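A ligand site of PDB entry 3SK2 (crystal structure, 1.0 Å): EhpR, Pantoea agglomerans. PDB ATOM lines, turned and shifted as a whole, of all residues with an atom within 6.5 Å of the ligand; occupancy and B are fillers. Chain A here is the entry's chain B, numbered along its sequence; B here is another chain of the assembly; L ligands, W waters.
An oxygen (O3) of the ligand lies within hydrogen-bond range of the indole nitrogen (NE1) of Trp 60, 2.9 Å away.
NE of Arg 45 is in salt-bridge range of O1 of the ligand, at 3.1 Å.
The backbone carbonyl oxygen of Leu 18 sits at hydrogen-bond distance from the backbone NH of Glu 75 of chain B, at 2.9 Å.
The side-chain hydroxyl (OG1) of Thr 43 is in hydrogen-bond range of the backbone carbonyl oxygen (O) of Tyr 46.
Water W4 bridges an oxygen (O2) of the ligand and the backbone carbonyl oxygen of Leu 131 of chain B.
Water W2 lies within hydrogen-bond range of O2 of the ligand (2.8 Å) and OH of Tyr 46 (2.9 Å).
Water W5 lies within hydrogen-bond range of an oxygen (O3) of the ligand and the indole nitrogen of Trp 60.
Water W1 lies within hydrogen-bond range of the side-chain hydroxyl (OG1) of Thr 43 (2.7 Å), the backbone NH (N) of Arg 45 (2.9 Å) and an oxygen (O1) of the ligand (3.1 Å).
Leu 18 touches the ligand.
CE2 of Phe 41 touches C6 of the ligand, at 3.7 Å.
Thr 43 touches the ligand.
CG of Tyr 46 touches N2 of the ligand, 3.4 Å away.
Val 111 of chain B touches the ligand (CG2 to C8, 3.4 Å).
Phe 112 of chain B touches the ligand (CD2 to O4, 3.3 Å).
Hydrophobic or aromatic side chains that line the ligand: Leu 18, Phe 41, Tyr 46, Trp 60, Val 111 of chain B and Phe 112 of chain B.
Within 4 Å of the ligand: Leu 18, Phe 41, Thr 43, Arg 45, Tyr 46, Trp 60, Val 111 of chain B and Phe 112 of chain B.
The nearest printed residue that does not touch the ligand is Leu 131 of chain B (4.1 Å).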
ATOM      1  N   LEU A  16      -4.653  18.952 -30.469  1.00  0.00           N
ATOM      2  CA  LEU A  16      -5.209  19.714 -29.395  1.00  0.00           C
ATOM      3  C   LEU A  16      -5.938  18.771 -28.486  1.00  0.00           C
ATOM      4  O   LEU A  16      -6.707  17.900 -28.937  1.00  0.00           O
ATOM      5  CB  LEU A  16      -6.128  20.788 -29.950  1.00  0.00           C
ATOM      6  CG  LEU A  16      -6.911  21.655 -28.960  1.00  0.00           C
ATOM      7  CD1 LEU A  16      -5.965  22.628 -28.201  1.00  0.00           C
ATOM      8  CD2 LEU A  16      -7.973  22.501 -29.738  1.00  0.00           C
ATOM      9  N   LEU A  18      -8.459  19.457 -25.425  1.00  0.00           N
ATOM     10  CA  LEU A  18      -9.202  20.574 -24.873  1.00  0.00           C
ATOM     11  C   LEU A  18     -10.134  20.063 -23.802  1.00  0.00           C
ATOM     12  O   LEU A  18     -10.828  19.034 -23.969  1.00  0.00           O
ATOM     13  CB  LEU A  18      -9.972  21.237 -25.977  1.00  0.00           C
ATOM     14  CG  LEU A  18     -10.741  22.471 -25.436  1.00  0.00           C
ATOM     15  CD1 LEU A  18     -10.593  23.594 -26.347  1.00  0.00           C
ATOM     16  CD2 LEU A  18     -12.112  22.089 -24.990  1.00  0.00           C
ATOM     17  N   PHE A  41      -0.655  31.017 -24.599  1.00  0.00           N
ATOM     18  CA  PHE A  41      -1.685  31.923 -25.101  1.00  0.00           C
ATOM     19  C   PHE A  41      -2.718  32.029 -24.019  1.00  0.00           C
ATOM     20  O   PHE A  41      -3.228  31.035 -23.531  1.00  0.00           O
ATOM     21  CB  PHE A  41      -2.315  31.400 -26.358  1.00  0.00           C
ATOM     22  CG  PHE A  41      -3.315  32.285 -27.003  1.00  0.00           C
ATOM     23  CD1 PHE A  41      -3.028  33.608 -27.340  1.00  0.00           C
ATOM     24  CD2 PHE A  41      -4.601  31.802 -27.248  1.00  0.00           C
ATOM     25  CE1 PHE A  41      -3.991  34.419 -28.000  1.00  0.00           C
ATOM     26  CE2 PHE A  41      -5.576  32.596 -27.922  1.00  0.00           C
ATOM     27  CZ  PHE A  41      -5.248  33.878 -28.272  1.00  0.00           C
ATOM     28  N   THR A  43      -6.242  34.123 -22.795  1.00  0.00           N
ATOM     29  CA  THR A  43      -7.409  34.980 -22.940  1.00  0.00           C
ATOM     30  C   THR A  43      -8.354  34.731 -21.799  1.00  0.00           C
ATOM     31  O   THR A  43      -8.212  33.726 -21.115  1.00  0.00           O
ATOM     32  CB  THR A  43      -8.093  34.743 -24.303  1.00  0.00           C
ATOM     33  OG1 THR A  43      -8.896  33.558 -24.259  1.00  0.00           O
ATOM     34  CG2 THR A  43      -7.155  34.545 -25.441  1.00  0.00           C
ATOM     35  N   PRO A  44      -9.368  35.573 -21.580  1.00  0.00           N
ATOM     36  CA  PRO A  44     -10.211  35.343 -20.390  1.00  0.00           C
ATOM     37  C   PRO A  44     -11.035  34.024 -20.413  1.00  0.00           C
ATOM     38  O   PRO A  44     -11.376  33.493 -19.371  1.00  0.00           O
ATOM     39  CB  PRO A  44     -11.101  36.550 -20.363  1.00  0.00           C
ATOM     40  CG  PRO A  44     -10.249  37.606 -20.983  1.00  0.00           C
ATOM     41  CD  PRO A  44      -9.567  36.924 -22.159  1.00  0.00           C
ATOM     42  N   ARG A  45     -11.344  33.499 -21.609  1.00  0.00           N
ATOM     43  CA  ARG A  45     -12.183  32.276 -21.748  1.00  0.00           C
ATOM     44  C   ARG A  45     -11.397  31.037 -22.219  1.00  0.00           C
ATOM     45  O   ARG A  45     -11.953  29.957 -22.234  1.00  0.00           O
ATOM     46  CB  ARG A  45     -13.368  32.485 -22.763  1.00  0.00           C
ATOM     47  CG  ARG A  45     -14.308  33.609 -22.377  1.00  0.00           C
ATOM     48  CD  ARG A  45     -15.184  34.029 -23.529  1.00  0.00           C
ATOM     49  NE  ARG A  45     -14.409  34.890 -24.379  1.00  0.00           N
ATOM     50  CZ  ARG A  45     -14.971  35.771 -25.182  1.00  0.00           C
ATOM     51  NH1 ARG A  45     -16.292  35.842 -25.260  1.00  0.00           N
ATOM     52  NH2 ARG A  45     -14.254  36.612 -25.879  1.00  0.00           N
ATOM     53  N   TYR A  46     -10.156  31.228 -22.653  1.00  0.00           N
ATOM     54  CA  TYR A  46      -9.404  30.147 -23.356  1.00  0.00           C
ATOM     55  C   TYR A  46      -7.928  30.357 -23.072  1.00  0.00           C
ATOM     56  O   TYR A  46      -7.385  31.438 -23.322  1.00  0.00           O
ATOM     57  CB  TYR A  46      -9.680  30.226 -24.870  1.00  0.00           C
ATOM     58  CG  TYR A  46      -8.844  29.284 -25.686  1.00  0.00           C
ATOM     59  CD1 TYR A  46      -9.229  27.950 -25.876  1.00  0.00           C
ATOM     60  CD2 TYR A  46      -7.641  29.679 -26.244  1.00  0.00           C
ATOM     61  CE1 TYR A  46      -8.415  27.070 -26.647  1.00  0.00           C
ATOM     62  CE2 TYR A  46      -6.830  28.821 -27.009  1.00  0.00           C
ATOM     63  CZ  TYR A  46      -7.222  27.529 -27.185  1.00  0.00           C
ATOM     64  OH  TYR A  46      -6.474  26.623 -27.918  1.00  0.00           O
ATOM     65  N   LEU A  56      -1.029  21.393 -28.452  1.00  0.00           N
ATOM     66  CA  LEU A  56      -1.430  22.207 -27.310  1.00  0.00           C
ATOM     67  C   LEU A  56      -2.384  21.444 -26.396  1.00  0.00           C
ATOM     68  O   LEU A  56      -3.135  20.566 -26.862  1.00  0.00           O
ATOM     69  CB  LEU A  56      -2.138  23.468 -27.783  1.00  0.00           C
ATOM     70  CG  LEU A  56      -1.328  24.424 -28.645  1.00  0.00           C
ATOM     71  CD1 LEU A  56      -2.263  25.494 -29.184  1.00  0.00           C
ATOM     72  CD2 LEU A  56      -0.185  25.024 -27.901  1.00  0.00           C
ATOM     73  N   ALA A  58      -5.452  22.760 -23.844  1.00  0.00           N
ATOM     74  CA  ALA A  58      -6.208  23.989 -23.596  1.00  0.00           C
ATOM     75  C   ALA A  58      -7.357  23.760 -22.654  1.00  0.00           C
ATOM     76  O   ALA A  58      -7.983  22.710 -22.601  1.00  0.00           O
ATOM     77  CB  ALA A  58      -6.699  24.580 -24.888  1.00  0.00           C
ATOM     78  N   TRP A  60     -11.030  25.767 -21.480  1.00  0.00           N
ATOM     79  CA  TRP A  60     -12.002  26.617 -22.137  1.00  0.00           C
ATOM     80  C   TRP A  60     -13.265  26.697 -21.299  1.00  0.00           C
ATOM     81  O   TRP A  60     -13.829  25.690 -20.932  1.00  0.00           O
ATOM     82  CB  TRP A  60     -12.371  26.006 -23.497  1.00  0.00           C
ATOM     83  CG  TRP A  60     -13.290  26.782 -24.356  1.00  0.00           C
ATOM     84  CD1 TRP A  60     -13.238  28.106 -24.587  1.00  0.00           C
ATOM     85  CD2 TRP A  60     -14.298  26.272 -25.229  1.00  0.00           C
ATOM     86  NE1 TRP A  60     -14.197  28.468 -25.505  1.00  0.00           N
ATOM     87  CE2 TRP A  60     -14.851  27.352 -25.922  1.00  0.00           C
ATOM     88  CE3 TRP A  60     -14.840  24.988 -25.446  1.00  0.00           C
ATOM     89  CZ2 TRP A  60     -15.881  27.206 -26.877  1.00  0.00           C
ATOM     90  CZ3 TRP A  60     -15.870  24.835 -26.378  1.00  0.00           C
ATOM     91  CH2 TRP A  60     -16.372  25.920 -27.077  1.00  0.00           C
ATOM     92  N   GLY A  62     -16.070  28.056 -22.562  1.00  0.00           N
ATOM     93  CA  GLY A  62     -17.174  28.128 -23.525  1.00  0.00           C
ATOM     94  C   GLY A  62     -17.885  26.827 -23.847  1.00  0.00           C
ATOM     95  O   GLY A  62     -18.793  26.778 -24.702  1.00  0.00           O
ATOM     96  N   GLU B  75     -12.740  17.567 -25.510  1.00  0.00           N
ATOM     97  CA  GLU B  75     -12.729  17.422 -26.952  1.00  0.00           C
ATOM     98  C   GLU B  75     -11.356  17.007 -27.398  1.00  0.00           C
ATOM     99  O   GLU B  75     -10.366  17.444 -26.856  1.00  0.00           O
ATOM    100  CB  GLU B  75     -13.101  18.764 -27.646  1.00  0.00           C
ATOM    101  CG  GLU B  75     -14.391  19.369 -27.251  1.00  0.00           C
ATOM    102  CD  GLU B  75     -14.646  20.713 -27.897  1.00  0.00           C
ATOM    103  OE1 GLU B  75     -13.710  21.263 -28.549  1.00  0.00           O
ATOM    104  OE2 GLU B  75     -15.797  21.227 -27.727  1.00  0.00           O
ATOM    105  N   MET B  79      -6.260  20.931 -35.225  1.00  0.00           N
ATOM    106  CA  MET B  79      -6.005  22.326 -35.655  1.00  0.00           C
ATOM    107  C   MET B  79      -5.362  22.304 -37.033  1.00  0.00           C
ATOM    108  O   MET B  79      -4.294  21.646 -37.206  1.00  0.00           O
ATOM    109  CB  MET B  79      -5.092  23.055 -34.665  1.00  0.00           C
ATOM    110  CG  MET B  79      -5.608  23.024 -33.282  1.00  0.00           C
ATOM    111  SD  MET B  79      -4.626  23.934 -32.067  1.00  0.00           S
ATOM    112  CE  MET B  79      -3.107  23.020 -32.028  1.00  0.00           C
ATOM    113  N   ASP B 110     -17.137  30.303 -35.037  1.00  0.00           N
ATOM    114  CA  ASP B 110     -17.180  30.535 -33.585  1.00  0.00           C
ATOM    115  C   ASP B 110     -16.349  31.776 -33.222  1.00  0.00           C
ATOM    116  O   ASP B 110     -15.858  32.433 -34.094  1.00  0.00           O
ATOM    117  CB  ASP B 110     -16.791  29.242 -32.811  1.00  0.00           C
ATOM    118  CG  ASP B 110     -17.390  29.155 -31.398  1.00  0.00           C
ATOM    119  OD1 ASP B 110     -17.398  30.153 -30.627  1.00  0.00           O
ATOM    120  OD2 ASP B 110     -17.735  27.983 -30.983  1.00  0.00           O
ATOM    121  N   VAL B 111     -16.046  31.990 -31.949  1.00  0.00           N
ATOM    122  CA  VAL B 111     -15.187  33.146 -31.573  1.00  0.00           C
ATOM    123  C   VAL B 111     -13.845  32.945 -31.943  1.00  0.00           C
ATOM    124  O   VAL B 111     -13.086  33.906 -31.887  1.00  0.00           O
ATOM    125  CB  VAL B 111     -15.256  33.541 -30.185  1.00  0.00           C
ATOM    126  CG1 VAL B 111     -16.706  34.052 -29.932  1.00  0.00           C
ATOM    127  CG2 VAL B 111     -14.819  32.502 -29.305  1.00  0.00           C
ATOM    128  N   PHE B 112     -13.468  31.772 -32.335  1.00  0.00           N
ATOM    129  CA  PHE B 112     -12.097  31.430 -32.787  1.00  0.00           C
ATOM    130  C   PHE B 112     -12.006  31.038 -34.290  1.00  0.00           C
ATOM    131  O   PHE B 112     -11.078  30.292 -34.753  1.00  0.00           O
ATOM    132  CB  PHE B 112     -11.512  30.357 -31.891  1.00  0.00           C
ATOM    133  CG  PHE B 112     -12.452  29.190 -31.700  1.00  0.00           C
ATOM    134  CD1 PHE B 112     -12.505  28.103 -32.580  1.00  0.00           C
ATOM    135  CD2 PHE B 112     -13.308  29.157 -30.661  1.00  0.00           C
ATOM    136  CE1 PHE B 112     -13.387  27.101 -32.405  1.00  0.00           C
ATOM    137  CE2 PHE B 112     -14.214  28.120 -30.459  1.00  0.00           C
ATOM    138  CZ  PHE B 112     -14.226  27.078 -31.342  1.00  0.00           C
ATOM    139  N   ARG B 127     -13.269  18.122 -32.514  1.00  0.00           N
ATOM    140  CA  ARG B 127     -13.407  19.463 -33.088  1.00  0.00           C
ATOM    141  C   ARG B 127     -12.328  19.710 -34.109  1.00  0.00           C
ATOM    142  O   ARG B 127     -11.137  19.488 -33.814  1.00  0.00           O
ATOM    143  CB  ARG B 127     -13.323  20.550 -31.981  1.00  0.00           C
ATOM    144  CG  ARG B 127     -13.428  21.948 -32.600  1.00  0.00           C
ATOM    145  CD  ARG B 127     -13.380  23.058 -31.541  1.00  0.00           C
ATOM    146  NE  ARG B 127     -14.422  22.977 -30.562  1.00  0.00           N
ATOM    147  CZ  ARG B 127     -15.695  23.403 -30.720  1.00  0.00           C
ATOM    148  NH1 ARG B 127     -16.076  24.046 -31.833  1.00  0.00           N
ATOM    149  NH2 ARG B 127     -16.574  23.230 -29.726  1.00  0.00           N
ATOM    150  N   CYS B 129     -10.661  22.903 -36.138  1.00  0.00           N
ATOM    151  CA  CYS B 129     -10.597  24.334 -35.937  1.00  0.00           C
ATOM    152  C   CYS B 129      -9.298  24.828 -36.549  1.00  0.00           C
ATOM    153  O   CYS B 129      -8.452  24.045 -36.934  1.00  0.00           O
ATOM    154  CB  CYS B 129     -10.759  24.667 -34.461  1.00  0.00           C
ATOM    155  SG  CYS B 129      -9.472  23.907 -33.377  1.00  0.00           S
ATOM    156  N   PRO B 130      -9.115  26.168 -36.598  1.00  0.00           N
ATOM    157  CA  PRO B 130      -7.868  26.676 -37.219  1.00  0.00           C
ATOM    158  C   PRO B 130      -6.701  26.941 -36.196  1.00  0.00           C
ATOM    159  O   PRO B 130      -7.026  27.229 -35.035  1.00  0.00           O
ATOM    160  CB  PRO B 130      -8.270  27.973 -37.936  1.00  0.00           C
ATOM    161  CG  PRO B 130      -9.678  28.178 -37.536  1.00  0.00           C
ATOM    162  CD  PRO B 130     -10.060  27.242 -36.404  1.00  0.00           C
ATOM    163  N   LEU B 131      -5.411  26.783 -36.582  1.00  0.00           N
ATOM    164  CA  LEU B 131      -4.284  27.130 -35.717  1.00  0.00           C
ATOM    165  C   LEU B 131      -4.414  28.585 -35.342  1.00  0.00           C
ATOM    166  O   LEU B 131      -4.161  28.991 -34.175  1.00  0.00           O
ATOM    167  CB  LEU B 131      -2.960  26.890 -36.394  1.00  0.00           C
ATOM    168  CG  LEU B 131      -2.507  25.456 -36.401  1.00  0.00           C
ATOM    169  CD1 LEU B 131      -1.357  25.288 -37.365  1.00  0.00           C
ATOM    170  CD2 LEU B 131      -2.078  25.076 -34.969  1.00  0.00           C
ATOM    171  N   ASP B 132      -4.719  29.380 -36.376  1.00  0.00           N
ATOM    172  CA  ASP B 132      -4.761  30.824 -36.446  1.00  0.00           C
ATOM    173  C   ASP B 132      -6.159  31.264 -36.891  1.00  0.00           C
ATOM    174  O   ASP B 132      -7.125  31.100 -36.151  1.00  0.00           O
ATOM    175  CB  ASP B 132      -3.777  31.273 -37.540  1.00  0.00           C
ATOM    176  CG  ASP B 132      -3.771  30.284 -38.774  1.00  0.00           C
ATOM    177  OD1 ASP B 132      -4.866  29.895 -39.263  1.00  0.00           O
ATOM    178  OD2 ASP B 132      -2.664  29.866 -39.222  1.00  0.00           O
ATOM    179  OXT ASP B 132      -6.318  31.809 -38.017  1.00  0.00           O
HETATM  180  C1  LIG L   1     -12.420  26.021 -28.443  1.00  0.00           C
HETATM  181  O1  LIG L   1     -13.165  32.729 -26.209  1.00  0.00           O
HETATM  182  O2  LIG L   1      -6.126  30.002 -30.721  1.00  0.00           O
HETATM  183  O3  LIG L   1     -13.055  30.602 -27.016  1.00  0.00           O
HETATM  184  C2  LIG L   1      -9.903  33.999 -28.214  1.00  0.00           C
HETATM  185  C3  LIG L   1     -11.010  33.523 -27.549  1.00  0.00           C
HETATM  186  C4  LIG L   1      -8.795  27.317 -30.665  1.00  0.00           C
HETATM  187  C5  LIG L   1      -9.929  26.869 -29.965  1.00  0.00           C
HETATM  188  C6  LIG L   1      -9.096  33.121 -28.887  1.00  0.00           C
HETATM  189  C7  LIG L   1      -7.168  29.142 -31.359  1.00  0.00           C
HETATM  190  N1  LIG L   1      -8.696  30.868 -29.603  1.00  0.00           N
HETATM  191  N2  LIG L   1     -10.891  29.952 -28.286  1.00  0.00           N
HETATM  192  O4  LIG L   1     -11.759  27.340 -28.412  1.00  0.00           O
HETATM  193  C8  LIG L   1     -12.556  31.806 -26.884  1.00  0.00           C
HETATM  194  C9  LIG L   1      -8.373  28.665 -30.544  1.00  0.00           C
HETATM  195  C10 LIG L   1     -10.633  27.751 -29.132  1.00  0.00           C
HETATM  196  C11 LIG L   1     -11.339  32.185 -27.593  1.00  0.00           C
HETATM  197  C12 LIG L   1      -9.446  31.764 -28.942  1.00  0.00           C
HETATM  198  C13 LIG L   1      -9.079  29.552 -29.744  1.00  0.00           C
HETATM  199  C14 LIG L   1     -10.565  31.276 -28.259  1.00  0.00           C
HETATM  200  C15 LIG L   1     -10.204  29.075 -29.040  1.00  0.00           C
HETATM  201  O   HOH W   1     -11.422  34.489 -24.375  1.00  0.00           O
HETATM  202  O   HOH W   2      -4.483  28.147 -29.417  1.00  0.00           O
HETATM  203  O   HOH W   3      -8.477  30.535 -34.247  1.00  0.00           O
HETATM  204  O   HOH W   4      -4.456  31.235 -32.403  1.00  0.00           O
HETATM  205  O   HOH W   5     -15.711  31.203 -25.914  1.00  0.00           O
